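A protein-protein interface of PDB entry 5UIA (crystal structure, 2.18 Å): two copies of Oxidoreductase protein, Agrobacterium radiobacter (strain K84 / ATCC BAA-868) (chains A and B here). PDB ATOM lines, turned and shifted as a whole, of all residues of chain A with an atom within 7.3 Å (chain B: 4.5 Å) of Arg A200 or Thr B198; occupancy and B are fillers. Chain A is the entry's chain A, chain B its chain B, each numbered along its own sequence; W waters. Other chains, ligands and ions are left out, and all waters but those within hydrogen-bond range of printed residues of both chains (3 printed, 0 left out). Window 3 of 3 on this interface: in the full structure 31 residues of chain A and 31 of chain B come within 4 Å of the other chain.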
ATOM      1  N   ILE A 176      -4.652  -4.433  26.399  1.00  0.00           N
ATOM      2  CA  ILE A 176      -5.099  -3.938  27.696  1.00  0.00           C
ATOM      3  C   ILE A 176      -4.524  -4.831  28.804  1.00  0.00           C
ATOM      4  O   ILE A 176      -4.029  -4.321  29.806  1.00  0.00           O
ATOM      5  CB  ILE A 176      -6.636  -3.837  27.842  1.00  0.00           C
ATOM      6  CG1 ILE A 176      -7.251  -2.953  26.744  1.00  0.00           C
ATOM      7  CG2 ILE A 176      -6.981  -3.264  29.216  1.00  0.00           C
ATOM      8  CD1 ILE A 176      -8.756  -3.090  26.611  1.00  0.00           C
ATOM      9  N   LEU A 197     -15.844   3.854  34.059  1.00  0.00           N
ATOM     10  CA  LEU A 197     -14.889   3.622  32.989  1.00  0.00           C
ATOM     11  C   LEU A 197     -15.607   3.256  31.680  1.00  0.00           C
ATOM     12  O   LEU A 197     -16.584   2.510  31.695  1.00  0.00           O
ATOM     13  CB  LEU A 197     -13.966   2.500  33.438  1.00  0.00           C
ATOM     14  CG  LEU A 197     -12.910   1.913  32.503  1.00  0.00           C
ATOM     15  CD1 LEU A 197     -11.776   1.315  33.336  1.00  0.00           C
ATOM     16  CD2 LEU A 197     -13.486   0.876  31.542  1.00  0.00           C
ATOM     17  N   THR A 198     -15.118   3.788  30.561  1.00  0.00           N
ATOM     18  CA  THR A 198     -15.636   3.457  29.228  1.00  0.00           C
ATOM     19  C   THR A 198     -14.470   3.196  28.281  1.00  0.00           C
ATOM     20  O   THR A 198     -13.503   3.955  28.272  1.00  0.00           O
ATOM     21  CB  THR A 198     -16.500   4.601  28.659  1.00  0.00           C
ATOM     22  OG1 THR A 198     -17.348   5.122  29.690  1.00  0.00           O
ATOM     23  CG2 THR A 198     -17.361   4.113  27.516  1.00  0.00           C
ATOM     24  N   ALA A 199     -14.561   2.134  27.484  1.00  0.00           N
ATOM     25  CA  ALA A 199     -13.428   1.677  26.686  1.00  0.00           C
ATOM     26  C   ALA A 199     -13.825   1.264  25.290  1.00  0.00           C
ATOM     27  O   ALA A 199     -14.948   0.823  25.058  1.00  0.00           O
ATOM     28  CB  ALA A 199     -12.733   0.510  27.373  1.00  0.00           C
ATOM     29  N   ARG A 200     -12.871   1.401  24.373  1.00  0.00           N
ATOM     30  CA  ARG A 200     -13.018   1.004  22.982  1.00  0.00           C
ATOM     31  C   ARG A 200     -11.739   0.308  22.572  1.00  0.00           C
ATOM     32  O   ARG A 200     -10.658   0.749  22.950  1.00  0.00           O
ATOM     33  CB  ARG A 200     -13.229   2.231  22.090  1.00  0.00           C
ATOM     34  CG  ARG A 200     -14.479   3.029  22.399  1.00  0.00           C
ATOM     35  CD  ARG A 200     -15.726   2.236  22.049  1.00  0.00           C
ATOM     36  NE  ARG A 200     -16.934   3.039  22.231  1.00  0.00           N
ATOM     37  CZ  ARG A 200     -17.585   3.202  23.381  1.00  0.00           C
ATOM     38  NH1 ARG A 200     -17.206   2.585  24.505  1.00  0.00           N
ATOM     39  NH2 ARG A 200     -18.655   3.985  23.400  1.00  0.00           N
ATOM     40  N   THR A 201     -11.871  -0.767  21.795  1.00  0.00           N
ATOM     41  CA  THR A 201     -10.730  -1.525  21.300  1.00  0.00           C
ATOM     42  C   THR A 201     -10.883  -1.891  19.827  1.00  0.00           C
ATOM     43  O   THR A 201     -11.981  -1.940  19.299  1.00  0.00           O
ATOM     44  CB  THR A 201     -10.507  -2.826  22.102  1.00  0.00           C
ATOM     45  OG1 THR A 201     -11.652  -3.666  21.972  1.00  0.00           O
ATOM     46  CG2 THR A 201     -10.267  -2.528  23.574  1.00  0.00           C
ATOM     47  N   LYS A 202      -9.746  -2.194  19.210  1.00  0.00           N
ATOM     48  CA  LYS A 202      -9.623  -2.407  17.782  1.00  0.00           C
ATOM     49  C   LYS A 202      -8.425  -3.331  17.517  1.00  0.00           C
ATOM     50  O   LYS A 202      -7.446  -3.280  18.257  1.00  0.00           O
ATOM     51  CB  LYS A 202      -9.374  -1.049  17.131  1.00  0.00           C
ATOM     52  CG  LYS A 202      -9.538  -1.030  15.633  1.00  0.00           C
ATOM     53  CD  LYS A 202      -9.394   0.374  15.067  1.00  0.00           C
ATOM     54  CE  LYS A 202     -10.522   1.309  15.491  1.00  0.00           C
ATOM     55  NZ  LYS A 202     -10.230   2.161  16.684  1.00  0.00           N
ATOM     56  N   GLU A 211      -6.566  -7.583  20.429  1.00  0.00           N
ATOM     57  CA  GLU A 211      -6.710  -6.133  20.253  1.00  0.00           C
ATOM     58  C   GLU A 211      -5.366  -5.442  20.534  1.00  0.00           C
ATOM     59  O   GLU A 211      -4.686  -5.750  21.521  1.00  0.00           O
ATOM     60  CB  GLU A 211      -7.869  -5.570  21.112  1.00  0.00           C
ATOM     61  CG  GLU A 211      -7.558  -5.111  22.538  1.00  0.00           C
ATOM     62  CD  GLU A 211      -7.136  -6.213  23.495  1.00  0.00           C
ATOM     63  OE1 GLU A 211      -7.242  -7.414  23.153  1.00  0.00           O
ATOM     64  OE2 GLU A 211      -6.691  -5.881  24.616  1.00  0.00           O
ATOM     65  N   VAL A 213      -5.110  -1.786  19.962  1.00  0.00           N
ATOM     66  CA  VAL A 213      -5.395  -0.371  20.187  1.00  0.00           C
ATOM     67  C   VAL A 213      -6.514  -0.335  21.224  1.00  0.00           C
ATOM     68  O   VAL A 213      -7.508  -1.043  21.075  1.00  0.00           O
ATOM     69  CB  VAL A 213      -5.851   0.341  18.895  1.00  0.00           C
ATOM     70  CG1 VAL A 213      -6.003   1.844  19.119  1.00  0.00           C
ATOM     71  CG2 VAL A 213      -4.886   0.066  17.737  1.00  0.00           C
ATOM     72  N   ALA A 214      -6.335   0.435  22.294  1.00  0.00           N
ATOM     73  CA  ALA A 214      -7.396   0.628  23.282  1.00  0.00           C
ATOM     74  C   ALA A 214      -7.412   2.072  23.755  1.00  0.00           C
ATOM     75  O   ALA A 214      -6.361   2.657  23.997  1.00  0.00           O
ATOM     76  CB  ALA A 214      -7.228  -0.323  24.463  1.00  0.00           C
ATOM     77  N   THR A 215      -8.613   2.635  23.862  1.00  0.00           N
ATOM     78  CA  THR A 215      -8.825   4.004  24.319  1.00  0.00           C
ATOM     79  C   THR A 215      -9.841   3.929  25.444  1.00  0.00           C
ATOM     80  O   THR A 215     -10.910   3.350  25.277  1.00  0.00           O
ATOM     81  CB  THR A 215      -9.356   4.910  23.184  1.00  0.00           C
ATOM     82  OG1 THR A 215      -8.495   4.811  22.045  1.00  0.00           O
ATOM     83  CG2 THR A 215      -9.425   6.372  23.631  1.00  0.00           C
ATOM     84  N   ILE A 216      -9.493   4.512  26.587  1.00  0.00           N
ATOM     85  CA  ILE A 216     -10.246   4.350  27.821  1.00  0.00           C
ATOM     86  C   ILE A 216     -10.482   5.733  28.445  1.00  0.00           C
ATOM     87  O   ILE A 216      -9.541   6.491  28.632  1.00  0.00           O
ATOM     88  CB  ILE A 216      -9.479   3.441  28.817  1.00  0.00           C
ATOM     89  CG1 ILE A 216      -9.058   2.125  28.144  1.00  0.00           C
ATOM     90  CG2 ILE A 216     -10.328   3.156  30.046  1.00  0.00           C
ATOM     91  CD1 ILE A 216      -8.348   1.142  29.056  1.00  0.00           C
ATOM     92  N   LEU A 217     -11.738   6.040  28.758  1.00  0.00           N
ATOM     93  CA  LEU A 217     -12.127   7.285  29.428  1.00  0.00           C
ATOM     94  C   LEU A 217     -12.428   6.992  30.905  1.00  0.00           C
ATOM     95  O   LEU A 217     -13.331   6.214  31.197  1.00  0.00           O
ATOM     96  CB  LEU A 217     -13.366   7.869  28.739  1.00  0.00           C
ATOM     97  CG  LEU A 217     -14.010   9.140  29.294  1.00  0.00           C
ATOM     98  CD1 LEU A 217     -13.048  10.309  29.187  1.00  0.00           C
ATOM     99  CD2 LEU A 217     -15.312   9.454  28.561  1.00  0.00           C
ATOM    100  N   ASP A 219     -13.505   8.173  34.832  1.00  0.00           N
ATOM    101  CA  ASP A 219     -14.066   9.117  35.810  1.00  0.00           C
ATOM    102  C   ASP A 219     -13.493   8.754  37.179  1.00  0.00           C
ATOM    103  O   ASP A 219     -13.848   7.725  37.752  1.00  0.00           O
ATOM    104  CB  ASP A 219     -15.585   9.038  35.812  1.00  0.00           C
ATOM    105  CG  ASP A 219     -16.154   9.010  34.412  1.00  0.00           C
ATOM    106  OD1 ASP A 219     -15.891   9.962  33.643  1.00  0.00           O
ATOM    107  OD2 ASP A 219     -16.847   8.026  34.063  1.00  0.00           O
ATOM    108  N   VAL A 228      -6.830   7.213  29.046  1.00  0.00           N
ATOM    109  CA  VAL A 228      -5.753   6.230  28.899  1.00  0.00           C
ATOM    110  C   VAL A 228      -5.829   5.676  27.473  1.00  0.00           C
ATOM    111  O   VAL A 228      -6.823   5.053  27.092  1.00  0.00           O
ATOM    112  CB  VAL A 228      -5.856   5.110  29.951  1.00  0.00           C
ATOM    113  CG1 VAL A 228      -4.830   4.031  29.686  1.00  0.00           C
ATOM    114  CG2 VAL A 228      -5.667   5.692  31.344  1.00  0.00           C
ATOM    115  N   VAL A 230      -3.651   3.502  24.507  1.00  0.00           N
ATOM    116  CA  VAL A 230      -2.538   2.605  24.253  1.00  0.00           C
ATOM    117  C   VAL A 230      -2.646   2.018  22.850  1.00  0.00           C
ATOM    118  O   VAL A 230      -3.757   1.776  22.358  1.00  0.00           O
ATOM    119  CB  VAL A 230      -2.460   1.475  25.314  1.00  0.00           C
ATOM    120  CG1 VAL A 230      -2.154   2.076  26.671  1.00  0.00           C
ATOM    121  CG2 VAL A 230      -3.743   0.664  25.386  1.00  0.00           C
ATOM    122  N   ALA A 329     -12.618  -2.697  31.314  1.00  0.00           N
ATOM    123  CA  ALA A 329     -12.372  -2.188  29.951  1.00  0.00           C
ATOM    124  C   ALA A 329     -12.753  -3.193  28.870  1.00  0.00           C
ATOM    125  O   ALA A 329     -13.343  -2.809  27.865  1.00  0.00           O
ATOM    126  CB  ALA A 329     -10.927  -1.744  29.776  1.00  0.00           C
ATOM    127  N   SER A 332     -16.625  -3.205  28.911  1.00  0.00           N
ATOM    128  CA  SER A 332     -17.073  -1.980  28.228  1.00  0.00           C
ATOM    129  C   SER A 332     -16.890  -2.056  26.707  1.00  0.00           C
ATOM    130  O   SER A 332     -17.800  -1.722  25.950  1.00  0.00           O
ATOM    131  CB  SER A 332     -16.326  -0.760  28.770  1.00  0.00           C
ATOM    132  OG  SER A 332     -16.884   0.441  28.274  1.00  0.00           O
ATOM    133  N   ALA A 333     -15.719  -2.519  26.275  1.00  0.00           N
ATOM    134  CA  ALA A 333     -15.386  -2.596  24.850  1.00  0.00           C
ATOM    135  C   ALA A 333     -16.331  -3.507  24.085  1.00  0.00           C
ATOM    136  O   ALA A 333     -16.720  -3.178  22.976  1.00  0.00           O
ATOM    137  CB  ALA A 333     -13.945  -3.053  24.662  1.00  0.00           C
ATOM    138  N   ALA A 334     -16.702  -4.634  24.689  1.00  0.00           N
ATOM    139  CA  ALA A 334     -17.634  -5.597  24.073  1.00  0.00           C
ATOM    140  C   ALA A 334     -19.098  -5.112  24.074  1.00  0.00           C
ATOM    141  O   ALA A 334     -19.767  -5.162  23.043  1.00  0.00           O
ATOM    142  CB  ALA A 334     -17.527  -6.957  24.765  1.00  0.00           C
ATOM    143  N   ASN A 335     -19.573  -4.642  25.228  1.00  0.00           N
ATOM    144  CA  ASN A 335     -20.974  -4.206  25.410  1.00  0.00           C
ATOM    145  C   ASN A 335     -21.268  -2.798  24.904  1.00  0.00           C
ATOM    146  O   ASN A 335     -22.425  -2.472  24.670  1.00  0.00           O
ATOM    147  CB  ASN A 335     -21.369  -4.251  26.895  1.00  0.00           C
ATOM    148  CG  ASN A 335     -21.309  -5.651  27.481  1.00  0.00           C
ATOM    149  OD1 ASN A 335     -21.574  -6.644  26.795  1.00  0.00           O
ATOM    150  ND2 ASN A 335     -20.966  -5.737  28.766  1.00  0.00           N
ATOM    151  N   GLY A 336     -20.237  -1.964  24.773  1.00  0.00           N
ATOM    152  CA  GLY A 336     -20.412  -0.549  24.449  1.00  0.00           C
ATOM    153  C   GLY A 336     -20.990   0.281  25.590  1.00  0.00           C
ATOM    154  O   GLY A 336     -21.493   1.375  25.353  1.00  0.00           O
ATOM    155  N   ARG A 337     -20.898  -0.227  26.824  1.00  0.00           N
ATOM    156  CA  ARG A 337     -21.483   0.419  28.003  1.00  0.00           C
ATOM    157  C   ARG A 337     -20.403   0.946  28.960  1.00  0.00           C
ATOM    158  O   ARG A 337     -19.306   0.388  29.055  1.00  0.00           O
ATOM    159  CB  ARG A 337     -22.397  -0.569  28.754  1.00  0.00           C
ATOM    160  CG  ARG A 337     -23.756  -0.813  28.102  1.00  0.00           C
ATOM    161  N   THR A 338     -20.730   2.028  29.661  1.00  0.00           N
ATOM    162  CA  THR A 338     -19.955   2.472  30.818  1.00  0.00           C
ATOM    163  C   THR A 338     -20.119   1.453  31.953  1.00  0.00           C
ATOM    164  O   THR A 338     -21.212   0.931  32.163  1.00  0.00           O
ATOM    165  CB  THR A 338     -20.401   3.875  31.275  1.00  0.00           C
ATOM    166  OG1 THR A 338     -20.124   4.806  30.228  1.00  0.00           O
ATOM    167  CG2 THR A 338     -19.672   4.327  32.541  1.00  0.00           C
ATOM    168  N   LEU B 197     -21.317   8.652  20.875  1.00  0.00           N
ATOM    169  CA  LEU B 197     -20.577   9.716  21.535  1.00  0.00           C
ATOM    170  C   LEU B 197     -20.720   9.595  23.057  1.00  0.00           C
ATOM    171  O   LEU B 197     -21.800   9.300  23.556  1.00  0.00           O
ATOM    172  CB  LEU B 197     -21.121  11.051  21.031  1.00  0.00           C
ATOM    173  CG  LEU B 197     -20.546  12.375  21.547  1.00  0.00           C
ATOM    174  CD1 LEU B 197     -20.621  13.450  20.465  1.00  0.00           C
ATOM    175  CD2 LEU B 197     -21.256  12.857  22.810  1.00  0.00           C
ATOM    176  N   THR B 198     -19.627   9.814  23.781  1.00  0.00           N
ATOM    177  CA  THR B 198     -19.649   9.861  25.245  1.00  0.00           C
ATOM    178  C   THR B 198     -18.852  11.077  25.697  1.00  0.00           C
ATOM    179  O   THR B 198     -17.760  11.301  25.190  1.00  0.00           O
ATOM    180  CB  THR B 198     -19.044   8.583  25.859  1.00  0.00           C
ATOM    181  OG1 THR B 198     -19.553   7.439  25.168  1.00  0.00           O
ATOM    182  CG2 THR B 198     -19.400   8.465  27.332  1.00  0.00           C
ATOM    183  N   ALA B 199     -19.382  11.837  26.655  1.00  0.00           N
ATOM    184  CA  ALA B 199     -18.792  13.118  27.060  1.00  0.00           C
ATOM    185  C   ALA B 199     -18.818  13.334  28.568  1.00  0.00           C
ATOM    186  O   ALA B 199     -19.721  12.863  29.250  1.00  0.00           O
ATOM    187  CB  ALA B 199     -19.520  14.266  26.367  1.00  0.00           C
ATOM    188  N   ARG B 200     -17.810  14.053  29.065  1.00  0.00           N
ATOM    189  CA  ARG B 200     -17.720  14.486  30.464  1.00  0.00           C
ATOM    190  C   ARG B 200     -17.412  15.977  30.494  1.00  0.00           C
ATOM    191  O   ARG B 200     -16.689  16.476  29.628  1.00  0.00           O
ATOM    192  CB  ARG B 200     -16.606  13.733  31.189  1.00  0.00           C
ATOM    193  CG  ARG B 200     -16.782  12.223  31.221  1.00  0.00           C
ATOM    194  CD  ARG B 200     -17.975  11.816  32.070  1.00  0.00           C
ATOM    195  NE  ARG B 200     -18.095  10.363  32.145  1.00  0.00           N
ATOM    196  CZ  ARG B 200     -18.778   9.591  31.301  1.00  0.00           C
ATOM    197  NH1 ARG B 200     -19.487  10.099  30.290  1.00  0.00           N
ATOM    198  NH2 ARG B 200     -18.773   8.277  31.495  1.00  0.00           N
ATOM    199  N   THR B 215     -14.273  16.606  27.874  1.00  0.00           N
ATOM    200  CA  THR B 215     -13.561  15.483  27.266  1.00  0.00           C
ATOM    201  C   THR B 215     -14.613  14.599  26.594  1.00  0.00           C
ATOM    202  O   THR B 215     -15.601  14.225  27.231  1.00  0.00           O
ATOM    203  CB  THR B 215     -12.778  14.676  28.324  1.00  0.00           C
ATOM    204  OG1 THR B 215     -11.885  15.548  29.029  1.00  0.00           O
ATOM    205  CG2 THR B 215     -11.966  13.564  27.683  1.00  0.00           C
ATOM    206  N   ILE B 216     -14.406  14.283  25.311  1.00  0.00           N
ATOM    207  CA  ILE B 216     -15.404  13.568  24.507  1.00  0.00           C
ATOM    208  C   ILE B 216     -14.766  12.398  23.754  1.00  0.00           C
ATOM    209  O   ILE B 216     -13.662  12.528  23.231  1.00  0.00           O
ATOM    210  CB  ILE B 216     -16.075  14.506  23.484  1.00  0.00           C
ATOM    211  CG1 ILE B 216     -16.690  15.730  24.189  1.00  0.00           C
ATOM    212  CG2 ILE B 216     -17.109  13.743  22.654  1.00  0.00           C
ATOM    213  CD1 ILE B 216     -17.218  16.799  23.253  1.00  0.00           C
ATOM    214  N   LEU B 217     -15.473  11.268  23.709  1.00  0.00           N
ATOM    215  CA  LEU B 217     -15.012  10.047  23.028  1.00  0.00           C
ATOM    216  C   LEU B 217     -15.956   9.742  21.859  1.00  0.00           C
ATOM    217  O   LEU B 217     -17.166   9.599  22.061  1.00  0.00           O
ATOM    218  CB  LEU B 217     -14.995   8.885  24.023  1.00  0.00           C
ATOM    219  CG  LEU B 217     -14.631   7.490  23.519  1.00  0.00           C
ATOM    220  CD1 LEU B 217     -13.165   7.441  23.134  1.00  0.00           C
ATOM    221  CD2 LEU B 217     -14.949   6.444  24.582  1.00  0.00           C
ATOM    222  N   ASP B 219     -17.091   7.452  18.500  1.00  0.00           N
ATOM    223  CA  ASP B 219     -17.080   6.248  17.668  1.00  0.00           C
ATOM    224  C   ASP B 219     -17.515   6.634  16.259  1.00  0.00           C
ATOM    225  O   ASP B 219     -18.688   6.922  16.020  1.00  0.00           O
ATOM    226  CB  ASP B 219     -17.996   5.193  18.257  1.00  0.00           C
ATOM    227  CG  ASP B 219     -17.702   4.943  19.721  1.00  0.00           C
ATOM    228  OD1 ASP B 219     -16.591   4.449  20.026  1.00  0.00           O
ATOM    229  OD2 ASP B 219     -18.567   5.259  20.568  1.00  0.00           O
ATOM    230  N   THR B 225     -11.714   5.577  16.227  1.00  0.00           N
ATOM    231  CA  THR B 225     -12.018   6.147  17.537  1.00  0.00           C
ATOM    232  C   THR B 225     -11.268   7.460  17.671  1.00  0.00           C
ATOM    233  O   THR B 225     -10.106   7.524  17.311  1.00  0.00           O
ATOM    234  CB  THR B 225     -11.578   5.208  18.674  1.00  0.00           C
ATOM    235  OG1 THR B 225     -12.163   3.914  18.487  1.00  0.00           O
ATOM    236  CG2 THR B 225     -12.009   5.767  20.041  1.00  0.00           C
ATOM    237  N   SER B 332     -24.980  13.487  27.164  1.00  0.00           N
ATOM    238  CA  SER B 332     -24.094  12.456  27.719  1.00  0.00           C
ATOM    239  C   SER B 332     -23.480  12.868  29.057  1.00  0.00           C
ATOM    240  O   SER B 332     -23.425  12.064  29.985  1.00  0.00           O
ATOM    241  CB  SER B 332     -22.969  12.135  26.728  1.00  0.00           C
ATOM    242  OG  SER B 332     -22.118  11.126  27.237  1.00  0.00           O
ATOM    243  N   ARG B 337     -24.239   8.767  30.137  1.00  0.00           N
ATOM    244  CA  ARG B 337     -24.520   7.682  29.190  1.00  0.00           C
ATOM    245  C   ARG B 337     -23.980   7.969  27.784  1.00  0.00           C
ATOM    246  O   ARG B 337     -23.769   9.125  27.407  1.00  0.00           O
ATOM    247  CB  ARG B 337     -26.031   7.426  29.123  1.00  0.00           C
ATOM    248  N   THR B 338     -23.756   6.900  27.020  1.00  0.00           N
ATOM    249  CA  THR B 338     -23.374   6.994  25.601  1.00  0.00           C
ATOM    250  C   THR B 338     -24.603   7.341  24.758  1.00  0.00           C
ATOM    251  O   THR B 338     -25.667   6.784  24.975  1.00  0.00           O
ATOM    252  CB  THR B 338     -22.759   5.668  25.104  1.00  0.00           C
ATOM    253  OG1 THR B 338     -21.571   5.404  25.847  1.00  0.00           O
ATOM    254  CG2 THR B 338     -22.396   5.722  23.625  1.00  0.00           C
HETATM  255  O   HOH W   1      -9.946   2.624  19.880  1.00  0.00           O
HETATM  256  O   HOH W   2     -18.484   7.068  22.599  1.00  0.00           O
HETATM  257  O   HOH W   3     -16.023   6.626  31.905  1.00  0.00           O
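The side-chain carboxylate (OD1) of Asp A219 lies within salt-bridge range of the guanidinium group (NE) of Arg B200 (2.7 Å). NZ of Lys A202 sits at hydrogen-bond distance from OG1 of Thr B225 (3.2 Å). OD1 of Asp B219 lies within salt-bridge range of NE of Arg A200, 2.6 Å away.
The backbone NH (N) of Leu A217 is in hydrogen-bond range of the backbone carbonyl oxygen (O) of Thr A198, at 2.8 Å. N of Arg A200 lies within hydrogen-bond range of O of Thr A215, at 2.9 Å. The backbone carbonyl oxygen (O) of Thr B198 is in hydrogen-bond range of the backbone NH (N) of Leu B217 (2.7 Å). N of Arg B200 is in hydrogen-bond range of O of Thr B215 (2.9 Å). N of Lys A202 is in hydrogen-bond range of O of Val A213. The side-chain hydroxyl of Thr A338 sits at hydrogen-bond distance from the side-chain hydroxyl of Thr A198.
Among the printed residues, merely in contact across the chains: Leu A217 with Thr B215 (3.7 Å), Thr A198 with Arg B200 (3.9 Å), Thr A215 with Leu B217 (3.9 Å), Thr A338 with Arg B200 (3.9 Å) and Arg A200 with Thr B198 (3.98 Å).
Printed residues of chain B within 4 Å of Thr A198: Arg B200. Of the printed residues of chain B, Arg A200 touches Thr B198 and Asp B219. Ala A329 touches none of the printed residues of chain B. Ser A332 touches none of the printed residues of chain B. Of the printed residues of chain A, Thr B198 touches Arg A200 (3.98 Å). Printed residues of chain A within 4 Å of Thr B215: Leu A217. Of the printed residues of chain A, Thr B225 touches Lys A202.
Of the 12 printed residues of chain B, 6 touch a printed residue of chain A. Of the 24 printed residues of chain A, 7 touch a printed residue of chain B. Printed residues of chain A that touch a printed residue of chain B: Thr A198, Arg A200, Lys A202, Thr A215, Leu A217, Asp A219 and Thr A338. Hydrophobic or aromatic side chains of chain A within 4 Å of the printed part of chain B: Leu A217. Along chain A the printed residues that touch a printed residue of chain B span positions 198 to 338. Among the printed residues, 8 pairs touch across the chains. Among the printed residues, Asp or Glu carboxylates within 4 Å of a Lys or Arg side-chain nitrogen of the other chain: Arg A200 with Asp B219 and Asp A219 with Arg B200.
Thr A198 touches Arg B200, and with the chains exchanged Arg A200 touches Thr B198. Arg A200 touches Asp B219, and with the chains exchanged Asp A219 touches Arg B200. Thr A215 touches Leu B217, and with the chains exchanged Leu A217 touches Thr B215. Thr A338 touches Arg B200, but with the chains exchanged Arg A200 does not touch Thr B338 (4.1 Å). Positions printed for both chains: 197, 198, 199, 200, 215, 216, 217, 219, 332, 337 and 338.
Water W3 lies within hydrogen-bond range of OD2 of Asp A219 (2.7 Å), O of Leu A217 (2.8 Å), OG1 of Thr A198 (3.0 Å) and NH2 of Arg B200 (3.2 Å). Water W2 lies within hydrogen-bond range of OD2 of Asp B219 (2.7 Å), OG1 of Thr B198 (2.8 Å), O of Leu B217 (2.9 Å) and NH2 of Arg A200 (3.2 Å). Water W1 lies within hydrogen-bond range of the side-chain hydroxyl of Thr B225, the side-chain amino group of Lys A202 and the side-chain hydroxyl of Thr A215.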
